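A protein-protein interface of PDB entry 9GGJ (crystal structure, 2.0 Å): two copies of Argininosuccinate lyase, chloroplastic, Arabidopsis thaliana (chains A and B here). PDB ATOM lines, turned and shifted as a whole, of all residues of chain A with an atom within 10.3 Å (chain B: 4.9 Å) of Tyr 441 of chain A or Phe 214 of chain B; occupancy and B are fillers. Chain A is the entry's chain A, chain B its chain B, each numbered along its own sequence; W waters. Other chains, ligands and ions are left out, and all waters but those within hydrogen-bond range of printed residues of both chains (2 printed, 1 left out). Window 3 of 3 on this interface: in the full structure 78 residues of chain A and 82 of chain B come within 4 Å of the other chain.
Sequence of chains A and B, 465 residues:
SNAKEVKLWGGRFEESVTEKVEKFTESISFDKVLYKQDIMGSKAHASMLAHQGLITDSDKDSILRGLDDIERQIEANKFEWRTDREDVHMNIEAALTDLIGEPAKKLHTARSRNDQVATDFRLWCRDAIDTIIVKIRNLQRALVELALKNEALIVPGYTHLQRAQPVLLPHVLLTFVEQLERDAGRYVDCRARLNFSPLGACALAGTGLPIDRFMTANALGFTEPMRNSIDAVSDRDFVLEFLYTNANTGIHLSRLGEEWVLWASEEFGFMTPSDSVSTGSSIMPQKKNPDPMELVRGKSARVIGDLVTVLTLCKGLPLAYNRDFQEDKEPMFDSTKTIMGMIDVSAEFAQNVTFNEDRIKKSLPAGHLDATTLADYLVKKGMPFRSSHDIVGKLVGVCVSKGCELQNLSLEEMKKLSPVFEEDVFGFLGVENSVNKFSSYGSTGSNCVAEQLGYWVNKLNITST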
ATOM      1  N   HIS A 171      32.848 -24.104 -31.887  1.00  0.00           N
ATOM      2  CA  HIS A 171      32.495 -25.192 -30.935  1.00  0.00           C
ATOM      3  C   HIS A 171      33.774 -25.897 -30.491  1.00  0.00           C
ATOM      4  O   HIS A 171      33.930 -26.137 -29.288  1.00  0.00           O
ATOM      5  CB  HIS A 171      31.507 -26.185 -31.549  1.00  0.00           C
ATOM      6  CG  HIS A 171      30.703 -26.931 -30.545  1.00  0.00           C
ATOM      7  ND1 HIS A 171      30.159 -26.315 -29.443  1.00  0.00           N
ATOM      8  CD2 HIS A 171      30.349 -28.216 -30.463  1.00  0.00           C
ATOM      9  CE1 HIS A 171      29.502 -27.209 -28.729  1.00  0.00           C
ATOM     10  NE2 HIS A 171      29.599 -28.368 -29.330  1.00  0.00           N
ATOM     11  N   GLU A 178      36.575 -24.399 -22.101  1.00  0.00           N
ATOM     12  CA  GLU A 178      35.912 -25.114 -21.017  1.00  0.00           C
ATOM     13  C   GLU A 178      36.919 -25.929 -20.190  1.00  0.00           C
ATOM     14  O   GLU A 178      36.790 -25.949 -18.988  1.00  0.00           O
ATOM     15  CB  GLU A 178      34.798 -26.033 -21.536  1.00  0.00           C
ATOM     16  CG  GLU A 178      33.514 -25.352 -21.993  1.00  0.00           C
ATOM     17  CD  GLU A 178      32.737 -24.517 -20.983  1.00  0.00           C
ATOM     18  OE1 GLU A 178      32.726 -24.821 -19.764  1.00  0.00           O
ATOM     19  OE2 GLU A 178      32.084 -23.553 -21.443  1.00  0.00           O
ATOM     20  N   LYS A 437      20.772 -27.484 -37.948  1.00  0.00           N
ATOM     21  CA  LYS A 437      19.696 -28.309 -37.399  1.00  0.00           C
ATOM     22  C   LYS A 437      20.018 -28.950 -36.038  1.00  0.00           C
ATOM     23  O   LYS A 437      19.105 -29.486 -35.403  1.00  0.00           O
ATOM     24  CB  LYS A 437      19.313 -29.424 -38.370  1.00  0.00           C
ATOM     25  CG  LYS A 437      18.627 -28.937 -39.628  1.00  0.00           C
ATOM     26  CD  LYS A 437      17.192 -28.485 -39.405  1.00  0.00           C
ATOM     27  CE  LYS A 437      16.631 -27.853 -40.621  1.00  0.00           C
ATOM     28  NZ  LYS A 437      15.217 -27.669 -40.329  1.00  0.00           N
ATOM     29  N   PHE A 438      21.286 -28.960 -35.600  1.00  0.00           N
ATOM     30  CA  PHE A 438      21.571 -29.339 -34.221  1.00  0.00           C
ATOM     31  C   PHE A 438      20.873 -28.355 -33.284  1.00  0.00           C
ATOM     32  O   PHE A 438      20.856 -27.164 -33.547  1.00  0.00           O
ATOM     33  CB  PHE A 438      23.070 -29.345 -33.912  1.00  0.00           C
ATOM     34  CG  PHE A 438      23.830 -30.462 -34.608  1.00  0.00           C
ATOM     35  CD1 PHE A 438      23.946 -31.719 -34.024  1.00  0.00           C
ATOM     36  CD2 PHE A 438      24.492 -30.236 -35.812  1.00  0.00           C
ATOM     37  CE1 PHE A 438      24.681 -32.729 -34.633  1.00  0.00           C
ATOM     38  CE2 PHE A 438      25.205 -31.260 -36.439  1.00  0.00           C
ATOM     39  CZ  PHE A 438      25.310 -32.506 -35.832  1.00  0.00           C
ATOM     40  N   SER A 439      20.267 -28.836 -32.197  1.00  0.00           N
ATOM     41  CA  SER A 439      19.482 -27.954 -31.360  1.00  0.00           C
ATOM     42  C   SER A 439      19.581 -28.310 -29.890  1.00  0.00           C
ATOM     43  O   SER A 439      19.099 -27.546 -29.090  1.00  0.00           O
ATOM     44  CB  SER A 439      18.076 -27.949 -31.787  1.00  0.00           C
ATOM     45  OG  SER A 439      17.572 -29.276 -31.697  1.00  0.00           O
ATOM     46  N   SER A 440      20.239 -29.406 -29.499  1.00  0.00           N
ATOM     47  CA  SER A 440      20.378 -29.711 -28.070  1.00  0.00           C
ATOM     48  C   SER A 440      21.357 -28.732 -27.397  1.00  0.00           C
ATOM     49  O   SER A 440      22.271 -28.172 -28.025  1.00  0.00           O
ATOM     50  CB  SER A 440      20.784 -31.136 -27.852  1.00  0.00           C
ATOM     51  OG  SER A 440      21.973 -31.477 -28.556  1.00  0.00           O
ATOM     52  N   TYR A 441      21.144 -28.500 -26.098  1.00  0.00           N
ATOM     53  CA  TYR A 441      22.022 -27.638 -25.338  1.00  0.00           C
ATOM     54  C   TYR A 441      23.441 -28.190 -25.463  1.00  0.00           C
ATOM     55  O   TYR A 441      23.649 -29.404 -25.416  1.00  0.00           O
ATOM     56  CB  TYR A 441      21.532 -27.536 -23.893  1.00  0.00           C
ATOM     57  CG  TYR A 441      22.328 -26.593 -23.021  1.00  0.00           C
ATOM     58  CD1 TYR A 441      22.105 -25.219 -23.088  1.00  0.00           C
ATOM     59  CD2 TYR A 441      23.270 -27.061 -22.118  1.00  0.00           C
ATOM     60  CE1 TYR A 441      22.812 -24.331 -22.291  1.00  0.00           C
ATOM     61  CE2 TYR A 441      24.021 -26.185 -21.348  1.00  0.00           C
ATOM     62  CZ  TYR A 441      23.776 -24.822 -21.433  1.00  0.00           C
ATOM     63  OH  TYR A 441      24.463 -23.920 -20.678  1.00  0.00           O
ATOM     64  N   GLY A 442      24.402 -27.277 -25.666  1.00  0.00           N
ATOM     65  CA  GLY A 442      25.812 -27.612 -25.757  1.00  0.00           C
ATOM     66  C   GLY A 442      26.167 -28.269 -27.088  1.00  0.00           C
ATOM     67  O   GLY A 442      27.330 -28.637 -27.279  1.00  0.00           O
ATOM     68  N   SER A 443      25.187 -28.402 -28.001  1.00  0.00           N
ATOM     69  CA  SER A 443      25.461 -28.904 -29.353  1.00  0.00           C
ATOM     70  C   SER A 443      26.274 -27.907 -30.193  1.00  0.00           C
ATOM     71  O   SER A 443      26.554 -26.794 -29.760  1.00  0.00           O
ATOM     72  CB  SER A 443      24.206 -29.240 -30.090  1.00  0.00           C
ATOM     73  OG  SER A 443      23.549 -28.064 -30.541  1.00  0.00           O
ATOM     74  N   THR A 444      26.644 -28.354 -31.409  1.00  0.00           N
ATOM     75  CA  THR A 444      27.385 -27.559 -32.380  1.00  0.00           C
ATOM     76  C   THR A 444      26.416 -26.713 -33.194  1.00  0.00           C
ATOM     77  O   THR A 444      26.838 -26.088 -34.150  1.00  0.00           O
ATOM     78  CB  THR A 444      28.231 -28.430 -33.315  1.00  0.00           C
ATOM     79  OG1 THR A 444      29.008 -27.536 -34.110  1.00  0.00           O
ATOM     80  CG2 THR A 444      27.365 -29.280 -34.229  1.00  0.00           C
ATOM     81  N   GLY A 445      25.130 -26.750 -32.865  1.00  0.00           N
ATOM     82  CA  GLY A 445      24.151 -25.991 -33.615  1.00  0.00           C
ATOM     83  C   GLY A 445      24.471 -24.495 -33.617  1.00  0.00           C
ATOM     84  O   GLY A 445      24.984 -23.940 -32.629  1.00  0.00           O
ATOM     85  N   SER A 446      24.116 -23.846 -34.725  1.00  0.00           N
ATOM     86  CA  SER A 446      24.493 -22.464 -34.949  1.00  0.00           C
ATOM     87  C   SER A 446      24.020 -21.586 -33.795  1.00  0.00           C
ATOM     88  O   SER A 446      24.783 -20.786 -33.268  1.00  0.00           O
ATOM     89  CB  SER A 446      23.941 -21.964 -36.310  1.00  0.00           C
ATOM     90  OG  SER A 446      24.352 -22.786 -37.409  1.00  0.00           O
ATOM     91  N   ASN A 447      22.758 -21.708 -33.410  1.00  0.00           N
ATOM     92  CA  ASN A 447      22.256 -20.871 -32.338  1.00  0.00           C
ATOM     93  C   ASN A 447      22.842 -21.277 -30.990  1.00  0.00           C
ATOM     94  O   ASN A 447      22.983 -20.442 -30.098  1.00  0.00           O
ATOM     95  CB  ASN A 447      20.743 -20.912 -32.245  1.00  0.00           C
ATOM     96  CG  ASN A 447      20.108 -20.176 -33.392  1.00  0.00           C
ATOM     97  OD1 ASN A 447      20.817 -19.604 -34.239  1.00  0.00           O
ATOM     98  ND2 ASN A 447      18.782 -20.165 -33.425  1.00  0.00           N
ATOM     99  N   CYS A 448      23.171 -22.565 -30.836  1.00  0.00           N
ATOM    100  CA  CYS A 448      23.702 -23.044 -29.575  1.00  0.00           C
ATOM    101  C   CYS A 448      25.096 -22.458 -29.346  1.00  0.00           C
ATOM    102  O   CYS A 448      25.430 -21.992 -28.255  1.00  0.00           O
ATOM    103  CB  CYS A 448      23.681 -24.565 -29.552  1.00  0.00           C
ATOM    104  SG  CYS A 448      22.022 -25.259 -29.786  1.00  0.00           S
ATOM    105  N   VAL A 449      25.922 -22.444 -30.392  1.00  0.00           N
ATOM    106  CA  VAL A 449      27.287 -21.977 -30.258  1.00  0.00           C
ATOM    107  C   VAL A 449      27.242 -20.475 -30.029  1.00  0.00           C
ATOM    108  O   VAL A 449      28.012 -19.973 -29.219  1.00  0.00           O
ATOM    109  CB  VAL A 449      28.086 -22.438 -31.488  1.00  0.00           C
ATOM    110  CG1 VAL A 449      29.451 -21.773 -31.603  1.00  0.00           C
ATOM    111  CG2 VAL A 449      28.252 -23.948 -31.474  1.00  0.00           C
ATOM    112  N   ALA A 450      26.259 -19.798 -30.650  1.00  0.00           N
ATOM    113  CA  ALA A 450      26.090 -18.353 -30.511  1.00  0.00           C
ATOM    114  C   ALA A 450      25.808 -18.034 -29.053  1.00  0.00           C
ATOM    115  O   ALA A 450      26.429 -17.114 -28.505  1.00  0.00           O
ATOM    116  CB  ALA A 450      24.998 -17.780 -31.413  1.00  0.00           C
ATOM    117  N   GLU A 451      24.895 -18.826 -28.456  1.00  0.00           N
ATOM    118  CA  GLU A 451      24.495 -18.641 -27.069  1.00  0.00           C
ATOM    119  C   GLU A 451      25.725 -18.746 -26.184  1.00  0.00           C
ATOM    120  O   GLU A 451      25.914 -17.922 -25.314  1.00  0.00           O
ATOM    121  CB  GLU A 451      23.415 -19.626 -26.634  1.00  0.00           C
ATOM    122  CG  GLU A 451      23.329 -19.767 -25.111  1.00  0.00           C
ATOM    123  CD  GLU A 451      22.070 -20.391 -24.547  1.00  0.00           C
ATOM    124  OE1 GLU A 451      21.198 -20.670 -25.388  1.00  0.00           O
ATOM    125  OE2 GLU A 451      21.953 -20.589 -23.311  1.00  0.00           O
ATOM    126  N   GLN A 452      26.549 -19.770 -26.434  1.00  0.00           N
ATOM    127  CA  GLN A 452      27.730 -20.067 -25.625  1.00  0.00           C
ATOM    128  C   GLN A 452      28.828 -19.032 -25.846  1.00  0.00           C
ATOM    129  O   GLN A 452      29.537 -18.676 -24.895  1.00  0.00           O
ATOM    130  CB  GLN A 452      28.287 -21.454 -25.918  1.00  0.00           C
ATOM    131  CG  GLN A 452      27.311 -22.578 -25.568  1.00  0.00           C
ATOM    132  CD  GLN A 452      27.016 -22.647 -24.085  1.00  0.00           C
ATOM    133  OE1 GLN A 452      27.846 -22.284 -23.233  1.00  0.00           O
ATOM    134  NE2 GLN A 452      25.845 -23.201 -23.786  1.00  0.00           N
ATOM    135  N   LEU A 453      28.915 -18.520 -27.081  1.00  0.00           N
ATOM    136  CA  LEU A 453      29.878 -17.471 -27.379  1.00  0.00           C
ATOM    137  C   LEU A 453      29.491 -16.178 -26.655  1.00  0.00           C
ATOM    138  O   LEU A 453      30.379 -15.451 -26.224  1.00  0.00           O
ATOM    139  CB  LEU A 453      30.009 -17.256 -28.881  1.00  0.00           C
ATOM    140  CG  LEU A 453      30.885 -18.258 -29.629  1.00  0.00           C
ATOM    141  CD1 LEU A 453      30.680 -18.186 -31.131  1.00  0.00           C
ATOM    142  CD2 LEU A 453      32.302 -17.960 -29.315  1.00  0.00           C
ATOM    143  N   TYR A 455      28.113 -16.004 -23.764  1.00  0.00           N
ATOM    144  CA  TYR A 455      28.401 -16.234 -22.361  1.00  0.00           C
ATOM    145  C   TYR A 455      29.873 -15.944 -22.058  1.00  0.00           C
ATOM    146  O   TYR A 455      30.175 -15.308 -21.047  1.00  0.00           O
ATOM    147  CB  TYR A 455      27.997 -17.681 -22.053  1.00  0.00           C
ATOM    148  CG  TYR A 455      28.546 -18.181 -20.735  1.00  0.00           C
ATOM    149  CD1 TYR A 455      27.851 -17.946 -19.557  1.00  0.00           C
ATOM    150  CD2 TYR A 455      29.773 -18.817 -20.650  1.00  0.00           C
ATOM    151  CE1 TYR A 455      28.342 -18.348 -18.331  1.00  0.00           C
ATOM    152  CE2 TYR A 455      30.272 -19.235 -19.422  1.00  0.00           C
ATOM    153  CZ  TYR A 455      29.549 -19.010 -18.261  1.00  0.00           C
ATOM    154  OH  TYR A 455      29.974 -19.391 -17.017  1.00  0.00           O
ATOM    155  N   TRP A 456      30.785 -16.408 -22.929  1.00  0.00           N
ATOM    156  CA  TRP A 456      32.218 -16.155 -22.780  1.00  0.00           C
ATOM    157  C   TRP A 456      32.610 -14.712 -23.097  1.00  0.00           C
ATOM    158  O   TRP A 456      33.520 -14.184 -22.477  1.00  0.00           O
ATOM    159  CB  TRP A 456      33.008 -17.127 -23.664  1.00  0.00           C
ATOM    160  CG  TRP A 456      32.953 -18.504 -23.077  1.00  0.00           C
ATOM    161  CD1 TRP A 456      32.220 -19.562 -23.497  1.00  0.00           C
ATOM    162  CD2 TRP A 456      33.594 -18.902 -21.842  1.00  0.00           C
ATOM    163  NE1 TRP A 456      32.405 -20.611 -22.630  1.00  0.00           N
ATOM    164  CE2 TRP A 456      33.243 -20.238 -21.614  1.00  0.00           C
ATOM    165  CE3 TRP A 456      34.470 -18.269 -20.948  1.00  0.00           C
ATOM    166  CZ2 TRP A 456      33.700 -20.933 -20.506  1.00  0.00           C
ATOM    167  CZ3 TRP A 456      34.947 -18.963 -19.871  1.00  0.00           C
ATOM    168  CH2 TRP A 456      34.531 -20.265 -19.631  1.00  0.00           C
ATOM    169  N   ASP B 212      15.737 -33.148 -23.798  1.00  0.00           N
ATOM    170  CA  ASP B 212      15.886 -32.196 -22.702  1.00  0.00           C
ATOM    171  C   ASP B 212      17.017 -32.648 -21.760  1.00  0.00           C
ATOM    172  O   ASP B 212      16.826 -33.476 -20.854  1.00  0.00           O
ATOM    173  CB  ASP B 212      14.555 -32.039 -21.988  1.00  0.00           C
ATOM    174  CG  ASP B 212      14.531 -30.989 -20.889  1.00  0.00           C
ATOM    175  OD1 ASP B 212      15.617 -30.604 -20.427  1.00  0.00           O
ATOM    176  OD2 ASP B 212      13.430 -30.554 -20.510  1.00  0.00           O
ATOM    177  N   ARG B 213      18.208 -32.090 -21.975  1.00  0.00           N
ATOM    178  CA  ARG B 213      19.399 -32.477 -21.246  1.00  0.00           C
ATOM    179  C   ARG B 213      19.354 -31.977 -19.807  1.00  0.00           C
ATOM    180  O   ARG B 213      20.131 -32.446 -18.987  1.00  0.00           O
ATOM    181  CB  ARG B 213      20.661 -31.907 -21.912  1.00  0.00           C
ATOM    182  CG  ARG B 213      20.998 -32.449 -23.296  1.00  0.00           C
ATOM    183  CD  ARG B 213      22.373 -31.949 -23.732  1.00  0.00           C
ATOM    184  NE  ARG B 213      23.455 -32.419 -22.860  1.00  0.00           N
ATOM    185  CZ  ARG B 213      24.513 -31.722 -22.427  1.00  0.00           C
ATOM    186  NH1 ARG B 213      24.852 -30.564 -22.965  1.00  0.00           N
ATOM    187  NH2 ARG B 213      25.294 -32.200 -21.473  1.00  0.00           N
ATOM    188  N   PHE B 214      18.494 -31.012 -19.493  1.00  0.00           N
ATOM    189  CA  PHE B 214      18.393 -30.497 -18.142  1.00  0.00           C
ATOM    190  C   PHE B 214      17.580 -31.477 -17.278  1.00  0.00           C
ATOM    191  O   PHE B 214      17.857 -31.672 -16.091  1.00  0.00           O
ATOM    192  CB  PHE B 214      17.805 -29.074 -18.188  1.00  0.00           C
ATOM    193  CG  PHE B 214      18.784 -28.012 -18.657  1.00  0.00           C
ATOM    194  CD1 PHE B 214      18.999 -27.783 -20.004  1.00  0.00           C
ATOM    195  CD2 PHE B 214      19.508 -27.263 -17.756  1.00  0.00           C
ATOM    196  CE1 PHE B 214      19.904 -26.811 -20.433  1.00  0.00           C
ATOM    197  CE2 PHE B 214      20.453 -26.342 -18.188  1.00  0.00           C
ATOM    198  CZ  PHE B 214      20.638 -26.100 -19.521  1.00  0.00           C
ATOM    199  N   MET B 215      16.541 -32.073 -17.881  1.00  0.00           N
ATOM    200  CA  MET B 215      15.716 -33.086 -17.234  1.00  0.00           C
ATOM    201  C   MET B 215      16.570 -34.276 -16.784  1.00  0.00           C
ATOM    202  O   MET B 215      16.501 -34.648 -15.609  1.00  0.00           O
ATOM    203  CB  MET B 215      14.602 -33.548 -18.181  1.00  0.00           C
ATOM    204  CG  MET B 215      13.757 -34.676 -17.652  1.00  0.00           C
ATOM    205  SD  MET B 215      12.286 -34.928 -18.671  1.00  0.00           S
ATOM    206  CE  MET B 215      11.535 -36.285 -17.751  1.00  0.00           C
ATOM    207  N   THR B 216      17.373 -34.863 -17.696  1.00  0.00           N
ATOM    208  CA  THR B 216      18.170 -36.028 -17.325  1.00  0.00           C
ATOM    209  C   THR B 216      19.239 -35.613 -16.312  1.00  0.00           C
ATOM    210  O   THR B 216      19.628 -36.397 -15.460  1.00  0.00           O
ATOM    211  CB  THR B 216      18.829 -36.708 -18.530  1.00  0.00           C
ATOM    212  OG1 THR B 216      19.500 -35.721 -19.311  1.00  0.00           O
ATOM    213  CG2 THR B 216      17.835 -37.374 -19.458  1.00  0.00           C
ATOM    214  N   ALA B 217      19.791 -34.408 -16.432  1.00  0.00           N
ATOM    215  CA  ALA B 217      20.800 -33.987 -15.479  1.00  0.00           C
ATOM    216  C   ALA B 217      20.202 -33.948 -14.070  1.00  0.00           C
ATOM    217  O   ALA B 217      20.837 -34.424 -13.131  1.00  0.00           O
ATOM    218  CB  ALA B 217      21.388 -32.647 -15.881  1.00  0.00           C
ATOM    219  N   ASN B 218      18.988 -33.392 -13.915  1.00  0.00           N
ATOM    220  CA  ASN B 218      18.365 -33.243 -12.609  1.00  0.00           C
ATOM    221  C   ASN B 218      18.013 -34.627 -12.070  1.00  0.00           C
ATOM    222  O   ASN B 218      18.285 -34.942 -10.926  1.00  0.00           O
ATOM    223  CB  ASN B 218      17.141 -32.334 -12.683  1.00  0.00           C
ATOM    224  CG  ASN B 218      17.480 -30.890 -12.969  1.00  0.00           C
ATOM    225  OD1 ASN B 218      18.627 -30.455 -12.798  1.00  0.00           O
ATOM    226  ND2 ASN B 218      16.483 -30.124 -13.388  1.00  0.00           N
ATOM    227  N   PRO B 225      23.685 -29.684 -17.108  1.00  0.00           N
ATOM    228  CA  PRO B 225      24.346 -30.245 -18.290  1.00  0.00           C
ATOM    229  C   PRO B 225      25.627 -29.472 -18.607  1.00  0.00           C
ATOM    230  O   PRO B 225      25.642 -28.250 -18.466  1.00  0.00           O
ATOM    231  CB  PRO B 225      23.326 -30.149 -19.424  1.00  0.00           C
ATOM    232  CG  PRO B 225      22.079 -29.511 -18.834  1.00  0.00           C
ATOM    233  CD  PRO B 225      22.365 -29.109 -17.397  1.00  0.00           C
ATOM    234  N   MET B 226      26.679 -30.184 -19.057  1.00  0.00           N
ATOM    235  CA  MET B 226      27.931 -29.599 -19.543  1.00  0.00           C
ATOM    236  C   MET B 226      27.664 -28.716 -20.757  1.00  0.00           C
ATOM    237  O   MET B 226      26.790 -29.062 -21.565  1.00  0.00           O
ATOM    238  CB  MET B 226      28.954 -30.684 -19.913  1.00  0.00           C
ATOM    239  CG  MET B 226      29.445 -31.464 -18.697  1.00  0.00           C
ATOM    240  SD  MET B 226      30.620 -32.783 -19.055  1.00  0.00           S
ATOM    241  CE  MET B 226      32.195 -31.950 -19.318  1.00  0.00           C
ATOM    242  N   ARG B 227      28.429 -27.608 -20.875  1.00  0.00           N
ATOM    243  CA  ARG B 227      28.133 -26.548 -21.830  1.00  0.00           C
ATOM    244  C   ARG B 227      28.684 -26.897 -23.207  1.00  0.00           C
ATOM    245  O   ARG B 227      28.439 -26.176 -24.164  1.00  0.00           O
ATOM    246  CB  ARG B 227      28.677 -25.180 -21.395  1.00  0.00           C
ATOM    247  CG  ARG B 227      27.756 -24.410 -20.459  1.00  0.00           C
ATOM    248  CD  ARG B 227      28.433 -23.263 -19.711  1.00  0.00           C
ATOM    249  NE  ARG B 227      27.507 -22.427 -18.936  1.00  0.00           N
ATOM    250  CZ  ARG B 227      26.691 -21.517 -19.443  1.00  0.00           C
ATOM    251  NH1 ARG B 227      26.739 -21.180 -20.725  1.00  0.00           N
ATOM    252  NH2 ARG B 227      25.844 -20.889 -18.642  1.00  0.00           N
HETATM  253  O   HOH W   1      24.338 -20.629 -21.385  1.00  0.00           O
HETATM  254  O   HOH W   2      30.595 -26.957 -18.576  1.00  0.00           O
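O of Tyr 441 of chain A is in hydrogen-bond range of NH1 of Arg 213 of chain B, 3.0 Å away.
The side-chain amide oxygen of Gln 452 of chain A sits at hydrogen-bond distance from the guanidinium group of Arg 227 of chain B, at 3.0 Å.
No position is printed for both chains.
Printed residues of chain B within 4 Å of Tyr 441 of chain A: Arg 213, Phe 214, Pro 225, Met 226 and Arg 227.
Of chain A, only Tyr 441 (3.6 Å) comes within 4 Å of Phe 214 of chain B.
No residue of chain A comes within 4 Å of Asp 212 of chain B.
Of chain A, only Tyr 441 (3.0 Å) comes within 4 Å of Arg 213 of chain B.
No residue of chain A comes within 4 Å of Ala 217 of chain B.
Of chain A, only Tyr 441 (3.9 Å) comes within 4 Å of Pro 225 of chain B.
Printed residues of chain B within 4 Å of Tyr 455 of chain A: Arg 227.
Printed residues of chain A within 4 Å of Arg 227 of chain B: Glu 178, Tyr 441, Gly 442, Gln 452 and Tyr 455.
Of the printed residues of chain B, Gln 452 of chain A touches Arg 227 (3.0 Å).
The nearest printed residue of chain B that does not touch Tyr 455 of chain A is Met 226 of chain B (9.9 Å).
Water W1 lies within hydrogen-bond range of the guanidinium group (NH1) of Arg 227 of chain B (2.6 Å), the side-chain carboxylate (OE2) of Glu 451 of chain A (3.1 Å) and the side-chain hydroxyl (OH) of Tyr 441 of chain A (3.4 Å).
Water W2 bridges N of Arg 227 of chain B (3.2 Å) and OE1 of Glu 178 of chain A (3.2 Å).
Among the printed residues, merely in contact across the chains: Tyr 441 of chain A with Arg 227 of chain B (3.3 Å), Gly 442 of chain A with Arg 227 of chain B (3.4 Å), Tyr 455 of chain A with Arg 227 of chain B (3.5 Å), Tyr 441 of chain A with Phe 214 of chain B (3.6 Å), Glu 178 of chain A with Arg 227 of chain B (3.8 Å), Tyr 441 of chain A with Pro 225 of chain B (3.9 Å) and Tyr 441 of chain A with Met 226 of chain B (3.999 Å).
The guanidinium group (NH1) of Arg 213 of chain B lies within hydrogen-bond range of the backbone carbonyl oxygen (O) of Met 226 of chain B (2.8 Å).
A ring nitrogen (NE2) of His 171 of chain A lies close to the backbone carbonyl oxygen of Gly 442 of chain A.
OH of Tyr 441 of chain A lies within hydrogen-bond range of NE2 of Gln 452 of chain A (3.5 Å).
The side-chain hydroxyl of Thr 216 of chain B sits at hydrogen-bond distance from the backbone carbonyl oxygen of Arg 213 of chain B (3.4 Å).
OD1 of Asp 212 of chain B is in hydrogen-bond range of N of Phe 214 of chain B, at 3.1 Å.
NE1 of Trp 456 of chain A is in hydrogen-bond range of OE2 of Glu 178 of chain A, at 3.2 Å.
Printed residues of chain A that touch a printed residue of chain B: Glu 178, Tyr 441, Gly 442, Gln 452 and Tyr 455.
Along chain A the printed residues that touch a printed residue of chain B span positions 178 to 455.
Of the 10 printed residues of chain B, 5 touch a printed residue of chain A.
Hydrophobic or aromatic side chains of chain B that line the printed part of chain A: Phe 214.
Among the printed residues, 9 pairs touch across the chains.
Among the printed residues, no Asp or Glu carboxylate lies within 4 Å of a Lys or Arg side-chain nitrogen of the other chain.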
